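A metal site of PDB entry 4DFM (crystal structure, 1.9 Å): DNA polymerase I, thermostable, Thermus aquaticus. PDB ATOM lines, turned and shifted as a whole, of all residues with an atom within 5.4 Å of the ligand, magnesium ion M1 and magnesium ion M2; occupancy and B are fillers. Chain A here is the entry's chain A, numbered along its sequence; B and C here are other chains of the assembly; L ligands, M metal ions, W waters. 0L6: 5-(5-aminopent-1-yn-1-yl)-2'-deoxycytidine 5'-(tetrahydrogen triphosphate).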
ATOM      1  N   ARG A 281      34.947  -2.732  -4.229  1.00  0.00           N
ATOM      2  CA  ARG A 281      33.792  -3.471  -3.723  1.00  0.00           C
ATOM      3  C   ARG A 281      33.665  -3.238  -2.215  1.00  0.00           C
ATOM      4  O   ARG A 281      34.656  -2.922  -1.530  1.00  0.00           O
ATOM      5  CB  ARG A 281      33.938  -4.976  -3.971  1.00  0.00           C
ATOM      6  CG  ARG A 281      33.522  -5.471  -5.362  1.00  0.00           C
ATOM      7  CD  ARG A 281      33.488  -6.988  -5.381  1.00  0.00           C
ATOM      8  NE  ARG A 281      32.801  -7.553  -6.530  1.00  0.00           N
ATOM      9  CZ  ARG A 281      32.564  -8.851  -6.673  1.00  0.00           C
ATOM     10  NH1 ARG A 281      32.981  -9.700  -5.745  1.00  0.00           N
ATOM     11  NH2 ARG A 281      31.924  -9.299  -7.743  1.00  0.00           N
ATOM     12  N   ASP A 318      19.039  -7.139  -9.218  1.00  0.00           N
ATOM     13  CA  ASP A 318      20.355  -7.645  -9.609  1.00  0.00           C
ATOM     14  C   ASP A 318      20.696  -7.182 -11.028  1.00  0.00           C
ATOM     15  O   ASP A 318      19.951  -7.472 -11.963  1.00  0.00           O
ATOM     16  CB  ASP A 318      20.338  -9.185  -9.527  1.00  0.00           C
ATOM     17  CG  ASP A 318      21.737  -9.813  -9.627  1.00  0.00           C
ATOM     18  OD1 ASP A 318      22.485  -9.459 -10.570  1.00  0.00           O
ATOM     19  OD2 ASP A 318      22.084 -10.653  -8.768  1.00  0.00           O
ATOM     20  N   TYR A 319      21.814  -6.471 -11.188  1.00  0.00           N
ATOM     21  CA  TYR A 319      22.267  -6.058 -12.516  1.00  0.00           C
ATOM     22  C   TYR A 319      22.573  -7.271 -13.393  1.00  0.00           C
ATOM     23  O   TYR A 319      23.246  -8.199 -12.957  1.00  0.00           O
ATOM     24  CB  TYR A 319      23.523  -5.181 -12.449  1.00  0.00           C
ATOM     25  CG  TYR A 319      23.281  -3.748 -12.038  1.00  0.00           C
ATOM     26  CD1 TYR A 319      22.777  -2.815 -12.937  1.00  0.00           C
ATOM     27  CD2 TYR A 319      23.610  -3.312 -10.765  1.00  0.00           C
ATOM     28  CE1 TYR A 319      22.568  -1.498 -12.565  1.00  0.00           C
ATOM     29  CE2 TYR A 319      23.413  -1.995 -10.381  1.00  0.00           C
ATOM     30  CZ  TYR A 319      22.883  -1.091 -11.287  1.00  0.00           C
ATOM     31  OH  TYR A 319      22.687   0.212 -10.904  1.00  0.00           O
ATOM     32  N   SER A 320      22.070  -7.239 -14.619  1.00  0.00           N
ATOM     33  CA  SER A 320      22.271  -8.332 -15.568  1.00  0.00           C
ATOM     34  C   SER A 320      23.643  -8.259 -16.247  1.00  0.00           C
ATOM     35  O   SER A 320      24.018  -7.209 -16.770  1.00  0.00           O
ATOM     36  CB  SER A 320      21.152  -8.309 -16.619  1.00  0.00           C
ATOM     37  OG  SER A 320      21.548  -8.952 -17.821  1.00  0.00           O
ATOM     38  N   GLN A 321      24.394  -9.371 -16.216  1.00  0.00           N
ATOM     39  CA  GLN A 321      25.678  -9.488 -16.906  1.00  0.00           C
ATOM     40  C   GLN A 321      26.559  -8.259 -16.687  1.00  0.00           C
ATOM     41  O   GLN A 321      27.164  -7.751 -17.632  1.00  0.00           O
ATOM     42  CB  GLN A 321      25.454  -9.710 -18.406  1.00  0.00           C
ATOM     43  CG  GLN A 321      24.350 -10.729 -18.753  1.00  0.00           C
ATOM     44  CD  GLN A 321      24.129 -10.888 -20.246  1.00  0.00           C
ATOM     45  OE1 GLN A 321      24.994 -11.387 -20.958  1.00  0.00           O
ATOM     46  NE2 GLN A 321      22.975 -10.444 -20.732  1.00  0.00           N
ATOM     47  N   ILE A 322      26.619  -7.781 -15.455  1.00  0.00           N
ATOM     48  CA  ILE A 322      27.145  -6.438 -15.199  1.00  0.00           C
ATOM     49  C   ILE A 322      28.592  -6.196 -15.649  1.00  0.00           C
ATOM     50  O   ILE A 322      28.881  -5.203 -16.310  1.00  0.00           O
ATOM     51  CB  ILE A 322      26.925  -5.979 -13.730  1.00  0.00           C
ATOM     52  CG1 ILE A 322      27.314  -4.509 -13.570  1.00  0.00           C
ATOM     53  CG2 ILE A 322      27.687  -6.860 -12.752  1.00  0.00           C
ATOM     54  CD1 ILE A 322      26.563  -3.568 -14.500  1.00  0.00           C
ATOM     55  N   GLU A 323      29.506  -7.097 -15.322  1.00  0.00           N
ATOM     56  CA  GLU A 323      30.893  -6.860 -15.698  1.00  0.00           C
ATOM     57  C   GLU A 323      31.113  -6.944 -17.209  1.00  0.00           C
ATOM     58  O   GLU A 323      31.997  -6.270 -17.747  1.00  0.00           O
ATOM     59  CB  GLU A 323      31.844  -7.746 -14.899  1.00  0.00           C
ATOM     60  CG  GLU A 323      31.925  -7.309 -13.435  1.00  0.00           C
ATOM     61  CD  GLU A 323      33.053  -7.981 -12.662  1.00  0.00           C
ATOM     62  OE1 GLU A 323      33.995  -8.482 -13.304  1.00  0.00           O
ATOM     63  OE2 GLU A 323      32.990  -8.002 -11.426  1.00  0.00           O
ATOM     64  N   LEU A 324      30.307  -7.745 -17.901  1.00  0.00           N
ATOM     65  CA  LEU A 324      30.406  -7.843 -19.358  1.00  0.00           C
ATOM     66  C   LEU A 324      29.952  -6.525 -19.999  1.00  0.00           C
ATOM     67  O   LEU A 324      30.583  -6.031 -20.922  1.00  0.00           O
ATOM     68  CB  LEU A 324      29.581  -9.007 -19.917  1.00  0.00           C
ATOM     69  CG  LEU A 324      30.012 -10.455 -19.647  1.00  0.00           C
ATOM     70  CD1 LEU A 324      29.168 -11.440 -20.464  1.00  0.00           C
ATOM     71  CD2 LEU A 324      31.496 -10.662 -19.926  1.00  0.00           C
ATOM     72  N   HIS A 347      25.720 -15.414 -21.069  1.00  0.00           N
ATOM     73  CA  HIS A 347      25.693 -16.523 -20.123  1.00  0.00           C
ATOM     74  C   HIS A 347      24.826 -17.672 -20.645  1.00  0.00           C
ATOM     75  O   HIS A 347      25.225 -18.833 -20.573  1.00  0.00           O
ATOM     76  CB  HIS A 347      25.192 -16.052 -18.760  1.00  0.00           C
ATOM     77  CG  HIS A 347      26.098 -15.079 -18.078  1.00  0.00           C
ATOM     78  ND1 HIS A 347      27.471 -15.105 -18.241  1.00  0.00           N
ATOM     79  CD2 HIS A 347      25.844 -14.036 -17.253  1.00  0.00           C
ATOM     80  CE1 HIS A 347      28.015 -14.131 -17.534  1.00  0.00           C
ATOM     81  NE2 HIS A 347      27.048 -13.464 -16.930  1.00  0.00           N
ATOM     82  N   ARG A 367      22.876 -21.988 -16.617  1.00  0.00           N
ATOM     83  CA  ARG A 367      23.331 -20.625 -16.854  1.00  0.00           C
ATOM     84  C   ARG A 367      24.339 -20.199 -15.800  1.00  0.00           C
ATOM     85  O   ARG A 367      25.362 -19.586 -16.124  1.00  0.00           O
ATOM     86  CB  ARG A 367      22.143 -19.673 -16.866  1.00  0.00           C
ATOM     87  CG  ARG A 367      22.500 -18.262 -17.293  1.00  0.00           C
ATOM     88  CD  ARG A 367      21.255 -17.410 -17.424  1.00  0.00           C
ATOM     89  NE  ARG A 367      21.597 -16.026 -17.734  1.00  0.00           N
ATOM     90  CZ  ARG A 367      21.983 -15.132 -16.823  1.00  0.00           C
ATOM     91  NH1 ARG A 367      22.083 -15.480 -15.549  1.00  0.00           N
ATOM     92  NH2 ARG A 367      22.271 -13.902 -17.196  1.00  0.00           N
ATOM     93  N   ARG A 368      24.061 -20.523 -14.542  1.00  0.00           N
ATOM     94  CA  ARG A 368      24.961 -20.217 -13.433  1.00  0.00           C
ATOM     95  C   ARG A 368      26.327 -20.871 -13.651  1.00  0.00           C
ATOM     96  O   ARG A 368      27.359 -20.255 -13.396  1.00  0.00           O
ATOM     97  CB  ARG A 368      24.373 -20.661 -12.095  1.00  0.00           C
ATOM     98  CG  ARG A 368      25.321 -20.494 -10.913  1.00  0.00           C
ATOM     99  CD  ARG A 368      24.734 -21.075  -9.639  1.00  0.00           C
ATOM    100  NE  ARG A 368      25.633 -20.950  -8.499  1.00  0.00           N
ATOM    101  CZ  ARG A 368      25.736 -19.869  -7.736  1.00  0.00           C
ATOM    102  NH1 ARG A 368      24.975 -18.808  -7.996  1.00  0.00           N
ATOM    103  NH2 ARG A 368      26.584 -19.837  -6.713  1.00  0.00           N
ATOM    104  N   LYS A 371      28.307 -18.914 -16.045  1.00  0.00           N
ATOM    105  CA  LYS A 371      28.833 -17.652 -15.534  1.00  0.00           C
ATOM    106  C   LYS A 371      30.289 -17.789 -15.140  1.00  0.00           C
ATOM    107  O   LYS A 371      31.132 -16.957 -15.495  1.00  0.00           O
ATOM    108  CB  LYS A 371      28.052 -17.173 -14.317  1.00  0.00           C
ATOM    109  CG  LYS A 371      26.701 -16.582 -14.620  1.00  0.00           C
ATOM    110  CD  LYS A 371      26.270 -15.695 -13.469  1.00  0.00           C
ATOM    111  CE  LYS A 371      24.804 -15.859 -13.175  1.00  0.00           C
ATOM    112  NZ  LYS A 371      24.366 -14.923 -12.101  1.00  0.00           N
ATOM    113  N   THR A 372      30.584 -18.843 -14.391  1.00  0.00           N
ATOM    114  CA  THR A 372      31.945 -19.100 -13.931  1.00  0.00           C
ATOM    115  C   THR A 372      32.878 -19.272 -15.127  1.00  0.00           C
ATOM    116  O   THR A 372      33.986 -18.760 -15.136  1.00  0.00           O
ATOM    117  CB  THR A 372      31.998 -20.330 -13.007  1.00  0.00           C
ATOM    118  OG1 THR A 372      31.213 -20.067 -11.833  1.00  0.00           O
ATOM    119  CG2 THR A 372      33.427 -20.647 -12.605  1.00  0.00           C
ATOM    120  N   PHE A 375      33.368 -15.672 -17.003  1.00  0.00           N
ATOM    121  CA  PHE A 375      34.289 -14.785 -16.298  1.00  0.00           C
ATOM    122  C   PHE A 375      35.667 -15.424 -16.078  1.00  0.00           C
ATOM    123  O   PHE A 375      36.693 -14.736 -16.130  1.00  0.00           O
ATOM    124  CB  PHE A 375      33.686 -14.297 -14.977  1.00  0.00           C
ATOM    125  CG  PHE A 375      32.425 -13.496 -15.176  1.00  0.00           C
ATOM    126  CD1 PHE A 375      32.453 -12.333 -15.934  1.00  0.00           C
ATOM    127  CD2 PHE A 375      31.227 -13.920 -14.642  1.00  0.00           C
ATOM    128  CE1 PHE A 375      31.295 -11.596 -16.136  1.00  0.00           C
ATOM    129  CE2 PHE A 375      30.062 -13.177 -14.845  1.00  0.00           C
ATOM    130  CZ  PHE A 375      30.106 -12.027 -15.602  1.00  0.00           C
ATOM    131  N   TYR A 379      39.030 -13.572 -17.486  1.00  0.00           N
ATOM    132  CA  TYR A 379      40.102 -13.126 -16.605  1.00  0.00           C
ATOM    133  C   TYR A 379      41.302 -14.077 -16.520  1.00  0.00           C
ATOM    134  O   TYR A 379      42.080 -14.020 -15.574  1.00  0.00           O
ATOM    135  CB  TYR A 379      39.543 -12.797 -15.223  1.00  0.00           C
ATOM    136  CG  TYR A 379      38.535 -11.673 -15.265  1.00  0.00           C
ATOM    137  CD1 TYR A 379      38.911 -10.389 -15.622  1.00  0.00           C
ATOM    138  CD2 TYR A 379      37.200 -11.900 -14.962  1.00  0.00           C
ATOM    139  CE1 TYR A 379      38.002  -9.350 -15.671  1.00  0.00           C
ATOM    140  CE2 TYR A 379      36.271 -10.870 -15.014  1.00  0.00           C
ATOM    141  CZ  TYR A 379      36.674  -9.599 -15.359  1.00  0.00           C
ATOM    142  OH  TYR A 379      35.765  -8.560 -15.407  1.00  0.00           O
ATOM    143  N   ASN A 458      41.519  -6.894 -14.251  1.00  0.00           N
ATOM    144  CA  ASN A 458      40.225  -7.168 -13.643  1.00  0.00           C
ATOM    145  C   ASN A 458      39.694  -5.958 -12.897  1.00  0.00           C
ATOM    146  O   ASN A 458      38.499  -5.664 -12.957  1.00  0.00           O
ATOM    147  CB  ASN A 458      40.316  -8.370 -12.692  1.00  0.00           C
ATOM    148  CG  ASN A 458      39.075  -8.529 -11.832  1.00  0.00           C
ATOM    149  OD1 ASN A 458      39.012  -8.013 -10.713  1.00  0.00           O
ATOM    150  ND2 ASN A 458      38.084  -9.231 -12.355  1.00  0.00           N
ATOM    151  N   GLN A 462      35.696  -4.869 -12.410  1.00  0.00           N
ATOM    152  CA  GLN A 462      35.026  -5.121 -11.133  1.00  0.00           C
ATOM    153  C   GLN A 462      34.803  -3.819 -10.379  1.00  0.00           C
ATOM    154  O   GLN A 462      33.723  -3.583  -9.823  1.00  0.00           O
ATOM    155  CB  GLN A 462      35.831  -6.108 -10.272  1.00  0.00           C
ATOM    156  CG  GLN A 462      35.130  -6.486  -8.971  1.00  0.00           C
ATOM    157  CD  GLN A 462      35.970  -7.387  -8.086  1.00  0.00           C
ATOM    158  OE1 GLN A 462      36.410  -6.968  -7.004  1.00  0.00           O
ATOM    159  NE2 GLN A 462      36.190  -8.620  -8.520  1.00  0.00           N
ATOM    160  N   VAL A 491      24.805  -7.126  -2.232  1.00  0.00           N
ATOM    161  CA  VAL A 491      25.681  -8.261  -2.542  1.00  0.00           C
ATOM    162  C   VAL A 491      26.327  -8.024  -3.905  1.00  0.00           C
ATOM    163  O   VAL A 491      26.025  -8.692  -4.894  1.00  0.00           O
ATOM    164  CB  VAL A 491      24.919  -9.618  -2.525  1.00  0.00           C
ATOM    165  CG1 VAL A 491      25.916 -10.791  -2.652  1.00  0.00           C
ATOM    166  CG2 VAL A 491      24.113  -9.752  -1.243  1.00  0.00           C
ATOM    167  N   ASP A 493      26.433  -6.776  -6.944  1.00  0.00           N
ATOM    168  CA  ASP A 493      25.631  -6.169  -7.997  1.00  0.00           C
ATOM    169  C   ASP A 493      24.158  -6.388  -7.730  1.00  0.00           C
ATOM    170  O   ASP A 493      23.322  -6.281  -8.636  1.00  0.00           O
ATOM    171  CB  ASP A 493      26.036  -6.687  -9.377  1.00  0.00           C
ATOM    172  CG  ASP A 493      25.467  -8.050  -9.681  1.00  0.00           C
ATOM    173  OD1 ASP A 493      25.386  -8.904  -8.766  1.00  0.00           O
ATOM    174  OD2 ASP A 493      25.086  -8.271 -10.857  1.00  0.00           O
ATOM    175  N   GLU A 494      23.842  -6.664  -6.471  1.00  0.00           N
ATOM    176  CA  GLU A 494      22.481  -6.960  -6.056  1.00  0.00           C
ATOM    177  C   GLU A 494      22.116  -6.117  -4.841  1.00  0.00           C
ATOM    178  O   GLU A 494      22.950  -5.880  -3.960  1.00  0.00           O
ATOM    179  CB  GLU A 494      22.354  -8.447  -5.709  1.00  0.00           C
ATOM    180  CG  GLU A 494      21.028  -8.846  -5.078  1.00  0.00           C
ATOM    181  CD  GLU A 494      20.995 -10.317  -4.687  1.00  0.00           C
ATOM    182  OE1 GLU A 494      21.991 -11.028  -4.948  1.00  0.00           O
ATOM    183  OE2 GLU A 494      19.967 -10.760  -4.134  1.00  0.00           O
ATOM    184  N   LYS A 539      14.249 -13.859  -5.545  1.00  0.00           N
ATOM    185  CA  LYS A 539      15.187 -13.917  -6.668  1.00  0.00           C
ATOM    186  C   LYS A 539      14.660 -14.739  -7.843  1.00  0.00           C
ATOM    187  O   LYS A 539      15.275 -14.781  -8.904  1.00  0.00           O
ATOM    188  CB  LYS A 539      16.559 -14.447  -6.234  1.00  0.00           C
ATOM    189  CG  LYS A 539      17.277 -13.567  -5.231  1.00  0.00           C
ATOM    190  CD  LYS A 539      18.801 -13.663  -5.372  1.00  0.00           C
ATOM    191  CE  LYS A 539      19.275 -12.969  -6.648  1.00  0.00           C
ATOM    192  NZ  LYS A 539      20.757 -13.023  -6.810  1.00  0.00           N
ATOM    193  P    DG B   4      43.662 -20.987 -13.407  1.00  0.00           P
ATOM    194  OP1  DG B   4      43.176 -21.743 -12.230  1.00  0.00           O
ATOM    195  OP2  DG B   4      43.717 -21.640 -14.734  1.00  0.00           O
ATOM    196  O5'  DG B   4      42.781 -19.649 -13.584  1.00  0.00           O
ATOM    197  C5'  DG B   4      42.762 -18.680 -12.554  1.00  0.00           C
ATOM    198  C4'  DG B   4      42.356 -17.336 -13.135  1.00  0.00           C
ATOM    199  O4'  DG B   4      41.156 -17.485 -13.931  1.00  0.00           O
ATOM    200  C3'  DG B   4      42.058 -16.273 -12.091  1.00  0.00           C
ATOM    201  O3'  DG B   4      43.239 -15.550 -11.876  1.00  0.00           O
ATOM    202  C2'  DG B   4      41.009 -15.403 -12.793  1.00  0.00           C
ATOM    203  C1'  DG B   4      40.260 -16.419 -13.662  1.00  0.00           C
ATOM    204  N9   DG B   4      39.067 -16.987 -13.041  1.00  0.00           N
ATOM    205  C8   DG B   4      38.826 -18.318 -12.763  1.00  0.00           C
ATOM    206  N7   DG B   4      37.651 -18.521 -12.224  1.00  0.00           N
ATOM    207  C5   DG B   4      37.089 -17.251 -12.134  1.00  0.00           C
ATOM    208  C6   DG B   4      35.841 -16.844 -11.622  1.00  0.00           C
ATOM    209  O6   DG B   4      34.952 -17.555 -11.140  1.00  0.00           O
ATOM    210  N1   DG B   4      35.663 -15.465 -11.725  1.00  0.00           N
ATOM    211  C2   DG B   4      36.582 -14.585 -12.237  1.00  0.00           C
ATOM    212  N2   DG B   4      36.238 -13.284 -12.238  1.00  0.00           N
ATOM    213  N3   DG B   4      37.766 -14.957 -12.713  1.00  0.00           N
ATOM    214  C4   DG B   4      37.952 -16.297 -12.635  1.00  0.00           C
ATOM    215  P    DC B   5      43.676 -15.119 -10.398  1.00  0.00           P
ATOM    216  OP1  DC B   5      45.072 -14.633 -10.464  1.00  0.00           O
ATOM    217  OP2  DC B   5      43.308 -16.221  -9.474  1.00  0.00           O
ATOM    218  O5'  DC B   5      42.734 -13.862 -10.074  1.00  0.00           O
ATOM    219  C5'  DC B   5      42.894 -12.655 -10.821  1.00  0.00           C
ATOM    220  C4'  DC B   5      41.729 -11.713 -10.567  1.00  0.00           C
ATOM    221  O4'  DC B   5      40.506 -12.328 -11.050  1.00  0.00           O
ATOM    222  C3'  DC B   5      41.438 -11.423  -9.095  1.00  0.00           C
ATOM    223  O3'  DC B   5      42.239 -10.363  -8.580  1.00  0.00           O
ATOM    224  C2'  DC B   5      39.973 -10.983  -9.165  1.00  0.00           C
ATOM    225  C1'  DC B   5      39.417 -11.939 -10.226  1.00  0.00           C
ATOM    226  N1   DC B   5      38.715 -13.163  -9.691  1.00  0.00           N
ATOM    227  C2   DC B   5      37.430 -13.037  -9.163  1.00  0.00           C
ATOM    228  O2   DC B   5      36.897 -11.918  -9.115  1.00  0.00           O
ATOM    229  N3   DC B   5      36.796 -14.142  -8.709  1.00  0.00           N
ATOM    230  C4   DC B   5      37.399 -15.334  -8.765  1.00  0.00           C
ATOM    231  N4   DC B   5      36.732 -16.399  -8.301  1.00  0.00           N
ATOM    232  C5   DC B   5      38.707 -15.478  -9.303  1.00  0.00           C
ATOM    233  C6   DC B   5      39.326 -14.375  -9.749  1.00  0.00           C
ATOM    234  P    DC C  11      27.216 -20.939  -2.723  1.00  0.00           P
ATOM    235  OP1  DC C  11      25.780 -21.253  -2.857  1.00  0.00           O
ATOM    236  OP2  DC C  11      28.198 -21.631  -3.582  1.00  0.00           O
ATOM    237  O5'  DC C  11      27.443 -19.365  -2.948  1.00  0.00           O
ATOM    238  C5'  DC C  11      26.643 -18.472  -2.197  1.00  0.00           C
ATOM    239  C4'  DC C  11      27.144 -17.036  -2.269  1.00  0.00           C
ATOM    240  O4'  DC C  11      28.501 -16.977  -1.756  1.00  0.00           O
ATOM    241  C3'  DC C  11      27.222 -16.416  -3.654  1.00  0.00           C
ATOM    242  O3'  DC C  11      25.924 -15.920  -4.041  1.00  0.00           O
ATOM    243  C2'  DC C  11      28.216 -15.283  -3.391  1.00  0.00           C
ATOM    244  C1'  DC C  11      29.192 -15.922  -2.400  1.00  0.00           C
ATOM    245  N1   DC C  11      30.407 -16.491  -3.024  1.00  0.00           N
ATOM    246  C2   DC C  11      31.494 -15.635  -3.234  1.00  0.00           C
ATOM    247  O2   DC C  11      31.376 -14.458  -2.894  1.00  0.00           O
ATOM    248  N3   DC C  11      32.640 -16.145  -3.789  1.00  0.00           N
ATOM    249  C4   DC C  11      32.700 -17.433  -4.127  1.00  0.00           C
ATOM    250  N4   DC C  11      33.840 -17.888  -4.668  1.00  0.00           N
ATOM    251  C5   DC C  11      31.601 -18.318  -3.923  1.00  0.00           C
ATOM    252  C6   DC C  11      30.483 -17.807  -3.363  1.00  0.00           C
ATOM    253  P   DDG C  12      25.805 -15.665  -5.621  1.00  0.00           P
ATOM    254  OP1 DDG C  12      24.376 -15.421  -5.240  1.00  0.00           O
ATOM    255  OP2 DDG C  12      25.927 -16.960  -6.368  1.00  0.00           O
ATOM    256  O5' DDG C  12      26.689 -14.444  -6.072  1.00  0.00           O
ATOM    257  C5' DDG C  12      26.406 -13.174  -5.551  1.00  0.00           C
ATOM    258  C4' DDG C  12      27.514 -12.215  -6.010  1.00  0.00           C
ATOM    259  O4' DDG C  12      28.726 -12.574  -5.468  1.00  0.00           O
ATOM    260  C3' DDG C  12      27.692 -12.224  -7.509  1.00  0.00           C
ATOM    261  C2' DDG C  12      29.096 -11.638  -7.574  1.00  0.00           C
ATOM    262  C1' DDG C  12      29.713 -12.205  -6.328  1.00  0.00           C
ATOM    263  N9  DDG C  12      30.505 -13.359  -6.640  1.00  0.00           N
ATOM    264  C8  DDG C  12      30.083 -14.677  -6.567  1.00  0.00           C
ATOM    265  N7  DDG C  12      31.128 -15.503  -6.935  1.00  0.00           N
ATOM    266  C5  DDG C  12      32.207 -14.660  -7.237  1.00  0.00           C
ATOM    267  C6  DDG C  12      33.573 -14.916  -7.678  1.00  0.00           C
ATOM    268  O6  DDG C  12      33.964 -16.217  -7.864  1.00  0.00           O
ATOM    269  N1  DDG C  12      34.436 -13.861  -7.895  1.00  0.00           N
ATOM    270  C2  DDG C  12      33.993 -12.528  -7.703  1.00  0.00           C
ATOM    271  N2  DDG C  12      34.890 -11.449  -7.923  1.00  0.00           N
ATOM    272  N3  DDG C  12      32.707 -12.273  -7.272  1.00  0.00           N
ATOM    273  C4  DDG C  12      31.821 -13.323  -7.047  1.00  0.00           C
HETATM  274  O2  0L6 L   1      33.841 -12.307 -11.438  1.00  0.00           O
HETATM  275  C2  0L6 L   1      32.881 -13.096 -11.246  1.00  0.00           C
HETATM  276  N3  0L6 L   1      33.075 -14.415 -11.236  1.00  0.00           N
HETATM  277  C4  0L6 L   1      32.058 -15.252 -11.026  1.00  0.00           C
HETATM  278  N4  0L6 L   1      32.274 -16.590 -11.015  1.00  0.00           N
HETATM  279  C5  0L6 L   1      30.796 -14.782 -10.814  1.00  0.00           C
HETATM  280  C29 0L6 L   1      29.874 -15.648 -10.605  1.00  0.00           C
HETATM  281  C30 0L6 L   1      29.028 -16.443 -10.409  1.00  0.00           C
HETATM  282  C31 0L6 L   1      27.969 -17.465 -10.234  1.00  0.00           C
HETATM  283  C32 0L6 L   1      28.523 -18.568  -9.315  1.00  0.00           C
HETATM  284  C33 0L6 L   1      28.991 -17.985  -7.979  1.00  0.00           C
HETATM  285  N34 0L6 L   1      30.051 -18.805  -7.433  1.00  0.00           N
HETATM  286  C6  0L6 L   1      30.545 -13.390 -10.803  1.00  0.00           C
HETATM  287  N1  0L6 L   1      31.585 -12.572 -11.022  1.00  0.00           N
HETATM  288  C1' 0L6 L   1      31.415 -11.107 -11.055  1.00  0.00           C
HETATM  289  O4' 0L6 L   1      30.281 -10.681 -10.283  1.00  0.00           O
HETATM  290  C2' 0L6 L   1      31.123 -10.755 -12.505  1.00  0.00           C
HETATM  291  C3' 0L6 L   1      29.607 -10.595 -12.508  1.00  0.00           C
HETATM  292  O3' 0L6 L   1      29.159  -9.757 -13.573  1.00  0.00           O
HETATM  293  C4' 0L6 L   1      29.336 -10.018 -11.136  1.00  0.00           C
HETATM  294  C5' 0L6 L   1      27.890 -10.211 -10.660  1.00  0.00           C
HETATM  295  O5' 0L6 L   1      27.594 -11.596 -10.537  1.00  0.00           O
HETATM  296  PA  0L6 L   1      26.150 -12.143 -11.000  1.00  0.00           P
HETATM  297  O1A 0L6 L   1      25.978 -13.520 -10.414  1.00  0.00           O
HETATM  298  O2A 0L6 L   1      25.062 -11.114 -10.768  1.00  0.00           O
HETATM  299  O3A 0L6 L   1      26.471 -12.341 -12.580  1.00  0.00           O
HETATM  300  PB  0L6 L   1      26.013 -11.337 -13.751  1.00  0.00           P
HETATM  301  O1B 0L6 L   1      25.528 -10.021 -13.180  1.00  0.00           O
HETATM  302  O2B 0L6 L   1      27.157 -11.292 -14.746  1.00  0.00           O
HETATM  303  O3B 0L6 L   1      24.820 -12.169 -14.475  1.00  0.00           O
HETATM  304  PG  0L6 L   1      23.252 -12.083 -14.108  1.00  0.00           P
HETATM  305  O1G 0L6 L   1      22.896 -13.510 -13.733  1.00  0.00           O
HETATM  306  O2G 0L6 L   1      23.144 -11.103 -12.956  1.00  0.00           O
HETATM  307  O3G 0L6 L   1      22.591 -11.644 -15.393  1.00  0.00           O
HETATM  308 MG    MG M   1      24.093  -9.747 -11.854  1.00  0.00          MG
HETATM  309 MG    MG M   2      24.232 -10.829  -8.514  1.00  0.00          MG
HETATM  310  O   HOH W   1      24.450 -10.711  -6.437  1.00  0.00           O
HETATM  311  O   HOH W   2      24.010 -12.950  -8.528  1.00  0.00           O
HETATM  312  O   HOH W   3      35.344  -9.786 -11.179  1.00  0.00           O
HETATM  313  O   HOH W   4      20.470 -10.169 -12.956  1.00  0.00           O
HETATM  314  O   HOH W   5      22.395 -13.123 -10.656  1.00  0.00           O
HETATM  315  O   HOH W   6      32.659 -18.701  -7.911  1.00  0.00           O
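DDG 12 of chain C touches magnesium ion M2 (C3' to MG, 3.9 Å).
Three residues have an atom within 4 Å of magnesium ion M2: Asp 318, Asp 493 and DDG 12 of chain C.
Magnesium ion M2 is bound by water W1, 2.1 Å away.
Magnesium ion M2 is bound by water W2 (2.1 Å).
OD2 of Asp 318 binds magnesium ion M2, 2.2 Å away.
The side-chain carboxylate (OD1) of Asp 493 binds magnesium ion M2, 2.3 Å away.
Magnesium ion M2 is bound by O2A of the ligand (2.4 Å).
Magnesium ion M2 has five donor atoms within binding distance.
Three residues have an atom within 4 Å of magnesium ion M1: Asp 318, Tyr 319 and Asp 493.
Along chain A the residues within 4 Å of magnesium ion M1 span positions 318 to 493.
The nearest printed residue that does not touch magnesium ion M1 is Ser 320 (4.2 Å).
NZ of Lys 371 is in salt-bridge range of O1G of the ligand (2.6 Å).
N1 of DG 4 of chain B lies within hydrogen-bond range of a nitrogen (N3) of the ligand (2.8 Å).
The guanidinium group (NH1) of Arg 367 lies within salt-bridge range of an oxygen (O1G) of the ligand, at 2.8 Å.
The backbone NH (N) of Gln 321 lies within hydrogen-bond range of an oxygen (O3G) of the ligand (3.0 Å).
NE2 of His 347 is in hydrogen-bond range of O2B of the ligand (3.1 Å).
N of Glu 323 sits at hydrogen-bond distance from O3' of the ligand.
The guanidinium group of Arg 281 sits at hydrogen-bond distance from an oxygen (O4') of the ligand.
N of Ile 322 sits close to O1B of the ligand, 3.4 Å away.
Magnesium ion M1 is bound by O1B of the ligand (2.0 Å), O2G of the ligand (2.0 Å), O2A of the ligand (2.0 Å), OD2 of Asp 493 (2.0 Å), OD1 of Asp 318 (2.1 Å) and O of Tyr 319 (2.1 Å).
Merely in contact with the ligand: Ser 320, Arg 368, Thr 372, Phe 375, DC 5 of chain B, DC 11 of chain C and DDG 12 of chain C.
Hydrophobic or aromatic side chains within 4 Å of the ligand: Ile 322, His 347 and Phe 375.
18 residues have an atom within 4 Å of the ligand: Arg 281, Asp 318, Tyr 319, Ser 320, Gln 321, Ile 322, Glu 323, His 347, Arg 367, Arg 368, Lys 371, Thr 372, Phe 375, Asp 493, DG 4 of chain B, DC 5 of chain B, DC 11 of chain C and DDG 12 of chain C.
Water W1 bridges OE1 of Glu 494 (2.9 Å) and O of Val 491 (3.0 Å).
Water W6 lies within hydrogen-bond range of N34 of the ligand (2.7 Å) and O6 of DDG 12 of chain C (2.8 Å).
Water W5 bridges NZ of Lys 371 (3.0 Å) and O1G of the ligand (3.1 Å).
OD2 of Asp 318 sits close to NZ of Lys 539 (3.3 Å).
NH1 of Arg 368 is in salt-bridge range of OP2 of DDG 12 of chain C, at 2.6 Å.
NH1 of Arg 281 lies within hydrogen-bond range of N3 of DDG 12 of chain C (3.0 Å).
N1 of DDG 12 of chain C lies close to N3 of DC 5 of chain B (2.5 Å).
N2 of DDG 12 of chain C lies within hydrogen-bond range of NE2 of Gln 462, at 3.2 Å.
The side-chain carboxylate (OE1) of Glu 323 is in hydrogen-bond range of the side-chain hydroxyl (OH) of Tyr 379, 2.7 Å away.
NH2 of Arg 368 is in salt-bridge range of OP2 of DC 11 of chain C, 3.95 Å away.
O2 of DC 5 of chain B is in hydrogen-bond range of NE2 of Gln 462.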
